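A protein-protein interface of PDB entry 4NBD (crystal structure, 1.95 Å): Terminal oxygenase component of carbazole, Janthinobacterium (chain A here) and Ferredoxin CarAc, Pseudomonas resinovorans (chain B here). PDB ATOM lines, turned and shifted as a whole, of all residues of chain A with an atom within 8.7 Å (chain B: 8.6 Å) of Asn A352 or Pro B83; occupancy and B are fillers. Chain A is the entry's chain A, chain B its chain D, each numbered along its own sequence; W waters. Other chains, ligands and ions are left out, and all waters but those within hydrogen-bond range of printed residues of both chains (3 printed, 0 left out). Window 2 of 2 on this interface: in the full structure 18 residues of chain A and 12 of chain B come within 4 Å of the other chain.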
ATOM      1  N   ILE A   8     -13.015  27.970   4.510  1.00  0.00           N
ATOM      2  CA  ILE A   8     -13.572  27.503   5.772  1.00  0.00           C
ATOM      3  C   ILE A   8     -12.658  27.891   6.936  1.00  0.00           C
ATOM      4  O   ILE A   8     -13.123  28.429   7.942  1.00  0.00           O
ATOM      5  CB  ILE A   8     -13.781  25.965   5.749  1.00  0.00           C
ATOM      6  CG1 ILE A   8     -14.922  25.625   4.779  1.00  0.00           C
ATOM      7  CG2 ILE A   8     -14.093  25.445   7.152  1.00  0.00           C
ATOM      8  CD1 ILE A   8     -15.167  24.141   4.576  1.00  0.00           C
ATOM      9  N   ARG A  11     -13.004  31.295   8.172  1.00  0.00           N
ATOM     10  CA  ARG A  11     -14.237  31.487   8.935  1.00  0.00           C
ATOM     11  C   ARG A  11     -14.138  31.110  10.417  1.00  0.00           C
ATOM     12  O   ARG A  11     -14.700  31.790  11.274  1.00  0.00           O
ATOM     13  CB  ARG A  11     -15.369  30.671   8.309  1.00  0.00           C
ATOM     14  CG  ARG A  11     -16.056  31.319   7.126  1.00  0.00           C
ATOM     15  CD  ARG A  11     -17.055  30.350   6.518  1.00  0.00           C
ATOM     16  NE  ARG A  11     -17.983  31.013   5.611  1.00  0.00           N
ATOM     17  CZ  ARG A  11     -19.015  31.752   6.004  1.00  0.00           C
ATOM     18  NH1 ARG A  11     -19.259  31.926   7.300  1.00  0.00           N
ATOM     19  NH2 ARG A  11     -19.799  32.325   5.098  1.00  0.00           N
ATOM     20  N   VAL A  12     -13.436  30.023  10.718  1.00  0.00           N
ATOM     21  CA  VAL A  12     -13.310  29.561  12.101  1.00  0.00           C
ATOM     22  C   VAL A  12     -12.096  30.140  12.818  1.00  0.00           C
ATOM     23  O   VAL A  12     -11.205  29.410  13.257  1.00  0.00           O
ATOM     24  CB  VAL A  12     -13.253  28.020  12.156  1.00  0.00           C
ATOM     25  CG1 VAL A  12     -14.600  27.444  11.758  1.00  0.00           C
ATOM     26  CG2 VAL A  12     -12.172  27.503  11.219  1.00  0.00           C
ATOM     27  N   PHE A 343     -22.234  15.121   8.410  1.00  0.00           N
ATOM     28  CA  PHE A 343     -22.295  16.563   8.588  1.00  0.00           C
ATOM     29  C   PHE A 343     -20.918  17.227   8.540  1.00  0.00           C
ATOM     30  O   PHE A 343     -20.773  18.319   8.004  1.00  0.00           O
ATOM     31  CB  PHE A 343     -22.994  16.880   9.911  1.00  0.00           C
ATOM     32  CG  PHE A 343     -23.355  18.329  10.087  1.00  0.00           C
ATOM     33  CD1 PHE A 343     -24.173  18.974   9.163  1.00  0.00           C
ATOM     34  CD2 PHE A 343     -22.920  19.035  11.206  1.00  0.00           C
ATOM     35  CE1 PHE A 343     -24.558  20.302   9.353  1.00  0.00           C
ATOM     36  CE2 PHE A 343     -23.298  20.359  11.408  1.00  0.00           C
ATOM     37  CZ  PHE A 343     -24.120  20.997  10.481  1.00  0.00           C
ATOM     38  N   TYR A 344     -19.907  16.556   9.080  1.00  0.00           N
ATOM     39  CA  TYR A 344     -18.548  17.104   9.113  1.00  0.00           C
ATOM     40  C   TYR A 344     -17.602  16.613   8.009  1.00  0.00           C
ATOM     41  O   TYR A 344     -16.511  17.153   7.848  1.00  0.00           O
ATOM     42  CB  TYR A 344     -17.930  16.820  10.493  1.00  0.00           C
ATOM     43  CG  TYR A 344     -18.562  17.640  11.605  1.00  0.00           C
ATOM     44  CD1 TYR A 344     -18.171  18.964  11.826  1.00  0.00           C
ATOM     45  CD2 TYR A 344     -19.590  17.116  12.395  1.00  0.00           C
ATOM     46  CE1 TYR A 344     -18.786  19.749  12.798  1.00  0.00           C
ATOM     47  CE2 TYR A 344     -20.213  17.895  13.374  1.00  0.00           C
ATOM     48  CZ  TYR A 344     -19.805  19.211  13.565  1.00  0.00           C
ATOM     49  OH  TYR A 344     -20.418  19.997  14.510  1.00  0.00           O
ATOM     50  N   ASP A 346     -17.512  17.003   4.768  1.00  0.00           N
ATOM     51  CA  ASP A 346     -17.116  17.983   3.764  1.00  0.00           C
ATOM     52  C   ASP A 346     -16.536  19.220   4.431  1.00  0.00           C
ATOM     53  O   ASP A 346     -16.305  20.235   3.776  1.00  0.00           O
ATOM     54  CB  ASP A 346     -18.323  18.384   2.918  1.00  0.00           C
ATOM     55  CG  ASP A 346     -19.533  18.727   3.767  1.00  0.00           C
ATOM     56  OD1 ASP A 346     -19.358  18.989   4.980  1.00  0.00           O
ATOM     57  OD2 ASP A 346     -20.657  18.741   3.219  1.00  0.00           O
ATOM     58  N   ASP A 347     -16.305  19.119   5.740  1.00  0.00           N
ATOM     59  CA  ASP A 347     -15.761  20.209   6.545  1.00  0.00           C
ATOM     60  C   ASP A 347     -16.768  21.337   6.778  1.00  0.00           C
ATOM     61  O   ASP A 347     -16.495  22.269   7.536  1.00  0.00           O
ATOM     62  CB  ASP A 347     -14.492  20.785   5.903  1.00  0.00           C
ATOM     63  CG  ASP A 347     -13.339  19.800   5.901  1.00  0.00           C
ATOM     64  OD1 ASP A 347     -13.105  19.161   6.948  1.00  0.00           O
ATOM     65  OD2 ASP A 347     -12.658  19.671   4.862  1.00  0.00           O
ATOM     66  N   LYS A 348     -17.934  21.245   6.140  1.00  0.00           N
ATOM     67  CA  LYS A 348     -18.969  22.272   6.274  1.00  0.00           C
ATOM     68  C   LYS A 348     -19.611  22.334   7.658  1.00  0.00           C
ATOM     69  O   LYS A 348     -20.029  23.404   8.105  1.00  0.00           O
ATOM     70  CB  LYS A 348     -20.069  22.058   5.229  1.00  0.00           C
ATOM     71  CG  LYS A 348     -19.622  22.227   3.781  1.00  0.00           C
ATOM     72  CD  LYS A 348     -19.159  23.645   3.496  1.00  0.00           C
ATOM     73  CE  LYS A 348     -19.334  23.995   2.024  1.00  0.00           C
ATOM     74  NZ  LYS A 348     -18.694  23.001   1.113  1.00  0.00           N
ATOM     75  N   GLY A 349     -19.706  21.189   8.328  1.00  0.00           N
ATOM     76  CA  GLY A 349     -20.303  21.160   9.651  1.00  0.00           C
ATOM     77  C   GLY A 349     -19.599  22.063  10.651  1.00  0.00           C
ATOM     78  O   GLY A 349     -20.223  22.551  11.597  1.00  0.00           O
ATOM     79  N   TRP A 350     -18.298  22.283  10.459  1.00  0.00           N
ATOM     80  CA  TRP A 350     -17.538  23.147  11.369  1.00  0.00           C
ATOM     81  C   TRP A 350     -18.014  24.594  11.242  1.00  0.00           C
ATOM     82  O   TRP A 350     -17.634  25.453  12.037  1.00  0.00           O
ATOM     83  CB  TRP A 350     -16.033  23.082  11.073  1.00  0.00           C
ATOM     84  CG  TRP A 350     -15.441  21.716  11.221  1.00  0.00           C
ATOM     85  CD1 TRP A 350     -14.996  20.901  10.220  1.00  0.00           C
ATOM     86  CD2 TRP A 350     -15.251  20.992  12.443  1.00  0.00           C
ATOM     87  NE1 TRP A 350     -14.543  19.713  10.741  1.00  0.00           N
ATOM     88  CE2 TRP A 350     -14.688  19.742  12.104  1.00  0.00           C
ATOM     89  CE3 TRP A 350     -15.504  21.278  13.794  1.00  0.00           C
ATOM     90  CZ2 TRP A 350     -14.374  18.776  13.063  1.00  0.00           C
ATOM     91  CZ3 TRP A 350     -15.194  20.320  14.749  1.00  0.00           C
ATOM     92  CH2 TRP A 350     -14.633  19.081  14.378  1.00  0.00           C
ATOM     93  N   VAL A 351     -18.834  24.866  10.229  1.00  0.00           N
ATOM     94  CA  VAL A 351     -19.369  26.209  10.042  1.00  0.00           C
ATOM     95  C   VAL A 351     -20.875  26.252  10.283  1.00  0.00           C
ATOM     96  O   VAL A 351     -21.385  27.195  10.881  1.00  0.00           O
ATOM     97  CB  VAL A 351     -19.095  26.745   8.616  1.00  0.00           C
ATOM     98  CG1 VAL A 351     -19.884  28.025   8.384  1.00  0.00           C
ATOM     99  CG2 VAL A 351     -17.610  27.025   8.439  1.00  0.00           C
ATOM    100  N   ASN A 352     -21.581  25.219   9.836  1.00  0.00           N
ATOM    101  CA  ASN A 352     -23.033  25.193   9.971  1.00  0.00           C
ATOM    102  C   ASN A 352     -23.638  24.681  11.280  1.00  0.00           C
ATOM    103  O   ASN A 352     -24.840  24.834  11.501  1.00  0.00           O
ATOM    104  CB  ASN A 352     -23.632  24.430   8.788  1.00  0.00           C
ATOM    105  CG  ASN A 352     -23.324  25.101   7.467  1.00  0.00           C
ATOM    106  OD1 ASN A 352     -23.149  26.318   7.412  1.00  0.00           O
ATOM    107  ND2 ASN A 352     -23.256  24.318   6.399  1.00  0.00           N
ATOM    108  N   GLU A 353     -22.818  24.090  12.146  1.00  0.00           N
ATOM    109  CA  GLU A 353     -23.300  23.573  13.434  1.00  0.00           C
ATOM    110  C   GLU A 353     -23.966  24.703  14.219  1.00  0.00           C
ATOM    111  O   GLU A 353     -23.542  25.848  14.123  1.00  0.00           O
ATOM    112  CB  GLU A 353     -22.119  23.037  14.260  1.00  0.00           C
ATOM    113  CG  GLU A 353     -21.088  24.129  14.580  1.00  0.00           C
ATOM    114  CD  GLU A 353     -19.799  23.610  15.217  1.00  0.00           C
ATOM    115  OE1 GLU A 353     -19.601  22.374  15.291  1.00  0.00           O
ATOM    116  OE2 GLU A 353     -18.975  24.454  15.634  1.00  0.00           O
ATOM    117  N   ILE A 354     -25.017  24.389  14.972  1.00  0.00           N
ATOM    118  CA  ILE A 354     -25.682  25.394  15.807  1.00  0.00           C
ATOM    119  C   ILE A 354     -25.521  24.918  17.248  1.00  0.00           C
ATOM    120  O   ILE A 354     -26.250  24.051  17.727  1.00  0.00           O
ATOM    121  CB  ILE A 354     -27.182  25.545  15.468  1.00  0.00           C
ATOM    122  CG1 ILE A 354     -27.333  26.150  14.073  1.00  0.00           C
ATOM    123  CG2 ILE A 354     -27.866  26.445  16.499  1.00  0.00           C
ATOM    124  CD1 ILE A 354     -28.770  26.381  13.660  1.00  0.00           C
ATOM    125  N   LEU A 355     -24.538  25.489  17.927  1.00  0.00           N
ATOM    126  CA  LEU A 355     -24.221  25.110  19.296  1.00  0.00           C
ATOM    127  C   LEU A 355     -25.129  25.739  20.341  1.00  0.00           C
ATOM    128  O   LEU A 355     -25.722  26.793  20.099  1.00  0.00           O
ATOM    129  CB  LEU A 355     -22.778  25.517  19.606  1.00  0.00           C
ATOM    130  CG  LEU A 355     -21.716  25.077  18.599  1.00  0.00           C
ATOM    131  CD1 LEU A 355     -20.340  25.573  19.058  1.00  0.00           C
ATOM    132  CD2 LEU A 355     -21.733  23.556  18.474  1.00  0.00           C
ATOM    133  N   CYS B  46     -24.083  35.666  19.737  1.00  0.00           N
ATOM    134  CA  CYS B  46     -24.454  35.390  18.353  1.00  0.00           C
ATOM    135  C   CYS B  46     -25.689  34.487  18.316  1.00  0.00           C
ATOM    136  O   CYS B  46     -25.762  33.498  19.049  1.00  0.00           O
ATOM    137  CB  CYS B  46     -23.288  34.714  17.633  1.00  0.00           C
ATOM    138  SG  CYS B  46     -23.583  34.393  15.883  1.00  0.00           S
ATOM    139  N   THR B  47     -26.655  34.820  17.465  1.00  0.00           N
ATOM    140  CA  THR B  47     -27.875  34.020  17.376  1.00  0.00           C
ATOM    141  C   THR B  47     -27.651  32.627  16.790  1.00  0.00           C
ATOM    142  O   THR B  47     -28.466  31.726  17.000  1.00  0.00           O
ATOM    143  CB  THR B  47     -28.974  34.736  16.548  1.00  0.00           C
ATOM    144  OG1 THR B  47     -28.505  34.974  15.216  1.00  0.00           O
ATOM    145  CG2 THR B  47     -29.349  36.051  17.197  1.00  0.00           C
ATOM    146  N   HIS B  48     -26.546  32.449  16.070  1.00  0.00           N
ATOM    147  CA  HIS B  48     -26.219  31.158  15.458  1.00  0.00           C
ATOM    148  C   HIS B  48     -25.520  30.197  16.423  1.00  0.00           C
ATOM    149  O   HIS B  48     -25.310  29.026  16.102  1.00  0.00           O
ATOM    150  CB  HIS B  48     -25.337  31.373  14.219  1.00  0.00           C
ATOM    151  CG  HIS B  48     -24.925  30.103  13.536  1.00  0.00           C
ATOM    152  ND1 HIS B  48     -23.695  29.515  13.733  1.00  0.00           N
ATOM    153  CD2 HIS B  48     -25.586  29.303  12.665  1.00  0.00           C
ATOM    154  CE1 HIS B  48     -23.614  28.410  13.014  1.00  0.00           C
ATOM    155  NE2 HIS B  48     -24.749  28.258  12.356  1.00  0.00           N
ATOM    156  N   GLY B  49     -25.162  30.680  17.608  1.00  0.00           N
ATOM    157  CA  GLY B  49     -24.486  29.806  18.550  1.00  0.00           C
ATOM    158  C   GLY B  49     -24.331  30.379  19.940  1.00  0.00           C
ATOM    159  O   GLY B  49     -25.290  30.897  20.522  1.00  0.00           O
ATOM    160  N   CYS B  65     -18.834  37.353  13.437  1.00  0.00           N
ATOM    161  CA  CYS B  65     -18.700  36.418  14.550  1.00  0.00           C
ATOM    162  C   CYS B  65     -17.381  35.650  14.440  1.00  0.00           C
ATOM    163  O   CYS B  65     -17.033  35.145  13.375  1.00  0.00           O
ATOM    164  CB  CYS B  65     -19.875  35.437  14.553  1.00  0.00           C
ATOM    165  SG  CYS B  65     -19.830  34.244  15.908  1.00  0.00           S
ATOM    166  N   PHE B  67     -16.598  32.771  15.703  1.00  0.00           N
ATOM    167  CA  PHE B  67     -16.774  31.319  15.646  1.00  0.00           C
ATOM    168  C   PHE B  67     -16.839  30.713  14.248  1.00  0.00           C
ATOM    169  O   PHE B  67     -15.976  29.917  13.875  1.00  0.00           O
ATOM    170  CB  PHE B  67     -18.038  30.910  16.411  1.00  0.00           C
ATOM    171  CG  PHE B  67     -17.825  30.698  17.885  1.00  0.00           C
ATOM    172  CD1 PHE B  67     -16.783  31.328  18.560  1.00  0.00           C
ATOM    173  CD2 PHE B  67     -18.701  29.889  18.607  1.00  0.00           C
ATOM    174  CE1 PHE B  67     -16.616  31.158  19.936  1.00  0.00           C
ATOM    175  CE2 PHE B  67     -18.544  29.712  19.982  1.00  0.00           C
ATOM    176  CZ  PHE B  67     -17.500  30.349  20.648  1.00  0.00           C
ATOM    177  N   HIS B  68     -17.861  31.089  13.481  1.00  0.00           N
ATOM    178  CA  HIS B  68     -18.048  30.528  12.147  1.00  0.00           C
ATOM    179  C   HIS B  68     -18.028  31.529  10.988  1.00  0.00           C
ATOM    180  O   HIS B  68     -18.239  31.147   9.835  1.00  0.00           O
ATOM    181  CB  HIS B  68     -19.360  29.738  12.111  1.00  0.00           C
ATOM    182  CG  HIS B  68     -19.516  28.768  13.243  1.00  0.00           C
ATOM    183  ND1 HIS B  68     -20.472  28.920  14.225  1.00  0.00           N
ATOM    184  CD2 HIS B  68     -18.845  27.631  13.545  1.00  0.00           C
ATOM    185  CE1 HIS B  68     -20.384  27.918  15.082  1.00  0.00           C
ATOM    186  NE2 HIS B  68     -19.404  27.120  14.692  1.00  0.00           N
ATOM    187  N   GLY B  69     -17.783  32.801  11.281  1.00  0.00           N
ATOM    188  CA  GLY B  69     -17.733  33.786  10.217  1.00  0.00           C
ATOM    189  C   GLY B  69     -19.055  34.450   9.869  1.00  0.00           C
ATOM    190  O   GLY B  69     -19.119  35.261   8.943  1.00  0.00           O
ATOM    191  N   GLY B  70     -20.116  34.103  10.593  1.00  0.00           N
ATOM    192  CA  GLY B  70     -21.402  34.725  10.331  1.00  0.00           C
ATOM    193  C   GLY B  70     -21.277  36.213  10.609  1.00  0.00           C
ATOM    194  O   GLY B  70     -20.320  36.644  11.264  1.00  0.00           O
ATOM    195  N   ALA B  71     -22.232  37.005  10.129  1.00  0.00           N
ATOM    196  CA  ALA B  71     -22.181  38.448  10.338  1.00  0.00           C
ATOM    197  C   ALA B  71     -23.560  39.069  10.551  1.00  0.00           C
ATOM    198  O   ALA B  71     -24.580  38.501  10.160  1.00  0.00           O
ATOM    199  CB  ALA B  71     -21.489  39.110   9.156  1.00  0.00           C
ATOM    200  N   PHE B  72     -23.571  40.245  11.169  1.00  0.00           N
ATOM    201  CA  PHE B  72     -24.806  40.977  11.454  1.00  0.00           C
ATOM    202  C   PHE B  72     -24.609  42.463  11.204  1.00  0.00           C
ATOM    203  O   PHE B  72     -23.512  42.993  11.398  1.00  0.00           O
ATOM    204  CB  PHE B  72     -25.208  40.815  12.924  1.00  0.00           C
ATOM    205  CG  PHE B  72     -25.613  39.426  13.301  1.00  0.00           C
ATOM    206  CD1 PHE B  72     -26.879  38.943  12.974  1.00  0.00           C
ATOM    207  CD2 PHE B  72     -24.735  38.599  13.995  1.00  0.00           C
ATOM    208  CE1 PHE B  72     -27.267  37.655  13.339  1.00  0.00           C
ATOM    209  CE2 PHE B  72     -25.112  37.309  14.364  1.00  0.00           C
ATOM    210  CZ  PHE B  72     -26.383  36.838  14.035  1.00  0.00           C
ATOM    211  N   PRO B  79     -29.061  39.647   9.834  1.00  0.00           N
ATOM    212  CA  PRO B  79     -27.952  38.804   9.381  1.00  0.00           C
ATOM    213  C   PRO B  79     -27.311  39.430   8.144  1.00  0.00           C
ATOM    214  O   PRO B  79     -28.010  39.990   7.296  1.00  0.00           O
ATOM    215  CB  PRO B  79     -28.637  37.482   9.063  1.00  0.00           C
ATOM    216  CG  PRO B  79     -29.736  37.433  10.066  1.00  0.00           C
ATOM    217  CD  PRO B  79     -30.282  38.843  10.024  1.00  0.00           C
ATOM    218  N   ALA B  80     -25.988  39.341   8.043  1.00  0.00           N
ATOM    219  CA  ALA B  80     -25.273  39.908   6.906  1.00  0.00           C
ATOM    220  C   ALA B  80     -24.442  38.856   6.178  1.00  0.00           C
ATOM    221  O   ALA B  80     -23.956  39.093   5.073  1.00  0.00           O
ATOM    222  CB  ALA B  80     -24.383  41.050   7.370  1.00  0.00           C
ATOM    223  N   SER B  81     -24.281  37.692   6.800  1.00  0.00           N
ATOM    224  CA  SER B  81     -23.515  36.607   6.197  1.00  0.00           C
ATOM    225  C   SER B  81     -23.888  35.282   6.838  1.00  0.00           C
ATOM    226  O   SER B  81     -24.125  35.220   8.046  1.00  0.00           O
ATOM    227  CB  SER B  81     -22.009  36.839   6.385  1.00  0.00           C
ATOM    228  OG  SER B  81     -21.589  38.056   5.798  1.00  0.00           O
ATOM    229  N   SER B  82     -23.945  34.225   6.032  1.00  0.00           N
ATOM    230  CA  SER B  82     -24.256  32.904   6.560  1.00  0.00           C
ATOM    231  C   SER B  82     -23.092  32.510   7.474  1.00  0.00           C
ATOM    232  O   SER B  82     -21.997  33.063   7.359  1.00  0.00           O
ATOM    233  CB  SER B  82     -24.405  31.890   5.419  1.00  0.00           C
ATOM    234  OG  SER B  82     -23.267  31.887   4.578  1.00  0.00           O
ATOM    235  N   PRO B  83     -23.307  31.545   8.383  1.00  0.00           N
ATOM    236  CA  PRO B  83     -24.546  30.789   8.600  1.00  0.00           C
ATOM    237  C   PRO B  83     -25.646  31.489   9.409  1.00  0.00           C
ATOM    238  O   PRO B  83     -26.647  30.860   9.750  1.00  0.00           O
ATOM    239  CB  PRO B  83     -24.046  29.536   9.304  1.00  0.00           C
ATOM    240  CG  PRO B  83     -22.980  30.103  10.200  1.00  0.00           C
ATOM    241  CD  PRO B  83     -22.236  31.053   9.272  1.00  0.00           C
ATOM    242  N   CYS B  84     -25.479  32.773   9.712  1.00  0.00           N
ATOM    243  CA  CYS B  84     -26.482  33.489  10.504  1.00  0.00           C
ATOM    244  C   CYS B  84     -27.778  33.771   9.745  1.00  0.00           C
ATOM    245  O   CYS B  84     -27.746  34.246   8.606  1.00  0.00           O
ATOM    246  CB  CYS B  84     -25.900  34.803  11.025  1.00  0.00           C
ATOM    247  SG  CYS B  84     -24.513  34.574  12.162  1.00  0.00           S
ATOM    248  N   THR B  85     -28.911  33.480  10.384  1.00  0.00           N
ATOM    249  CA  THR B  85     -30.226  33.699   9.780  1.00  0.00           C
ATOM    250  C   THR B  85     -31.229  34.335  10.745  1.00  0.00           C
ATOM    251  O   THR B  85     -32.231  34.910  10.316  1.00  0.00           O
ATOM    252  CB  THR B  85     -30.841  32.379   9.261  1.00  0.00           C
ATOM    253  OG1 THR B  85     -30.932  31.436  10.338  1.00  0.00           O
ATOM    254  CG2 THR B  85     -29.996  31.791   8.144  1.00  0.00           C
ATOM    255  N   VAL B  86     -30.963  34.232  12.044  1.00  0.00           N
ATOM    256  CA  VAL B  86     -31.854  34.793  13.056  1.00  0.00           C
ATOM    257  C   VAL B  86     -31.427  36.205  13.453  1.00  0.00           C
ATOM    258  O   VAL B  86     -30.316  36.419  13.940  1.00  0.00           O
ATOM    259  CB  VAL B  86     -31.891  33.907  14.329  1.00  0.00           C
ATOM    260  CG1 VAL B  86     -32.826  34.516  15.364  1.00  0.00           C
ATOM    261  CG2 VAL B  86     -32.350  32.503  13.970  1.00  0.00           C
HETATM  262  O   HOH W   1     -13.783  29.379  15.623  1.00  0.00           O
HETATM  263  O   HOH W   2     -23.072  27.564  16.400  1.00  0.00           O
HETATM  264  O   HOH W   3     -14.835  34.392  11.658  1.00  0.00           O
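Of the printed residues of chain B, Val A351 touches His B48 (3.3 Å), His B68 (3.4 Å) and Pro B83 (3.4 Å).
Asn A352 touches just these residues of chain B: His B48 (3.5 Å) and Pro B83 (3.8 Å).
Of the printed residues of chain B, Leu A355 touches Gly B49.
Of the printed residues of chain A, Gly B49 touches Leu A355 (3.6 Å).
Ala B71 touches none of the printed residues of chain A.
Pro B83 touches three residues of chain A.
Val B86 touches none of the printed residues of chain A.
The nearest residue of chain B that does not touch Asn A352 is His B68 (5.2 Å).
The nearest residue of chain A that does not touch Pro B83 is Glu A353 (5.8 Å).
The nearest printed residue of chain B that does not touch Val A12 is His B68 (4.6 Å).
Of the 15 printed residues of chain A, 8 touch a printed residue of chain B.
Printed residues of chain A that touch a printed residue of chain B: Arg A11, Val A12, Trp A350, Val A351, Asn A352, Glu A353, Ile A354 and Leu A355.
Hydrophobic or aromatic side chains of chain A within 4 Å of the printed part of chain B: Val A12, Val A351 and Ile A354.
Hydrophobic or aromatic side chains of chain B within 4 Å of the printed part of chain A: His B48, His B68 and Pro B83.
Among the printed residues, 16 pairs touch across the chains.
Among the printed residues, no Asp or Glu carboxylate lies within 4 Å of a Lys or Arg side-chain nitrogen of the other chain.
SG of Cys B65 sits close to N of Phe B67 (3.6 Å).
SG of Cys B46 sits close to N of His B48 (3.5 Å).
The side-chain carboxylate (OE1) of Glu A353 lies within hydrogen-bond range of the side-chain hydroxyl (OH) of Tyr A344.
CD of Pro B83 touches NH1 of Arg A11 (3.7 Å).
CA of Val A12 touches O of Phe B67, at 3.2 Å.
CD2 of His B68 touches O of Trp A350 (2.9 Å).
O of Val A351 touches CE1 of His B48 (3.3 Å).
His B68 touches Val A351 (CG to O, 3.4 Å).
Val A351 touches Pro B83.
NE2 of His B48 touches O of Asn A352, 3.5 Å away.
Asn A352 touches Pro B83.
His B48 touches Ile A354.
Leu A355 touches Gly B49.
Water W3 lies within hydrogen-bond range of O of Arg A11 (2.6 Å), O of Cys B65 (2.9 Å) and N of Gly B69 (3.4 Å).
Water W2 lies within hydrogen-bond range of O of His B48 (2.7 Å), O of Glu A353 (2.9 Å) and N of Leu A355 (3.0 Å).
Water W1 bridges the backbone carbonyl oxygen (O) of Phe B67 (2.9 Å) and the backbone carbonyl oxygen (O) of Val A12 (3.5 Å).
The backbone carbonyl oxygen of Arg A11 is in hydrogen-bond range of the backbone NH of Gly B69 (3.2 Å).
O of Glu A353 sits close to NE2 of His B48, 3.2 Å away.
O of Ser B82 is in hydrogen-bond range of NH1 of Arg A11 (3.0 Å).
A ring nitrogen (NE2) of His B68 sits at hydrogen-bond distance from the side-chain carboxylate (OE2) of Glu A353 (2.9 Å).
The backbone carbonyl oxygen (O) of Arg A11 lies close to the backbone carbonyl oxygen (O) of Phe B67 (3.4 Å).
O of His B68 lies within hydrogen-bond range of NH1 of Arg A11, at 2.8 Å.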
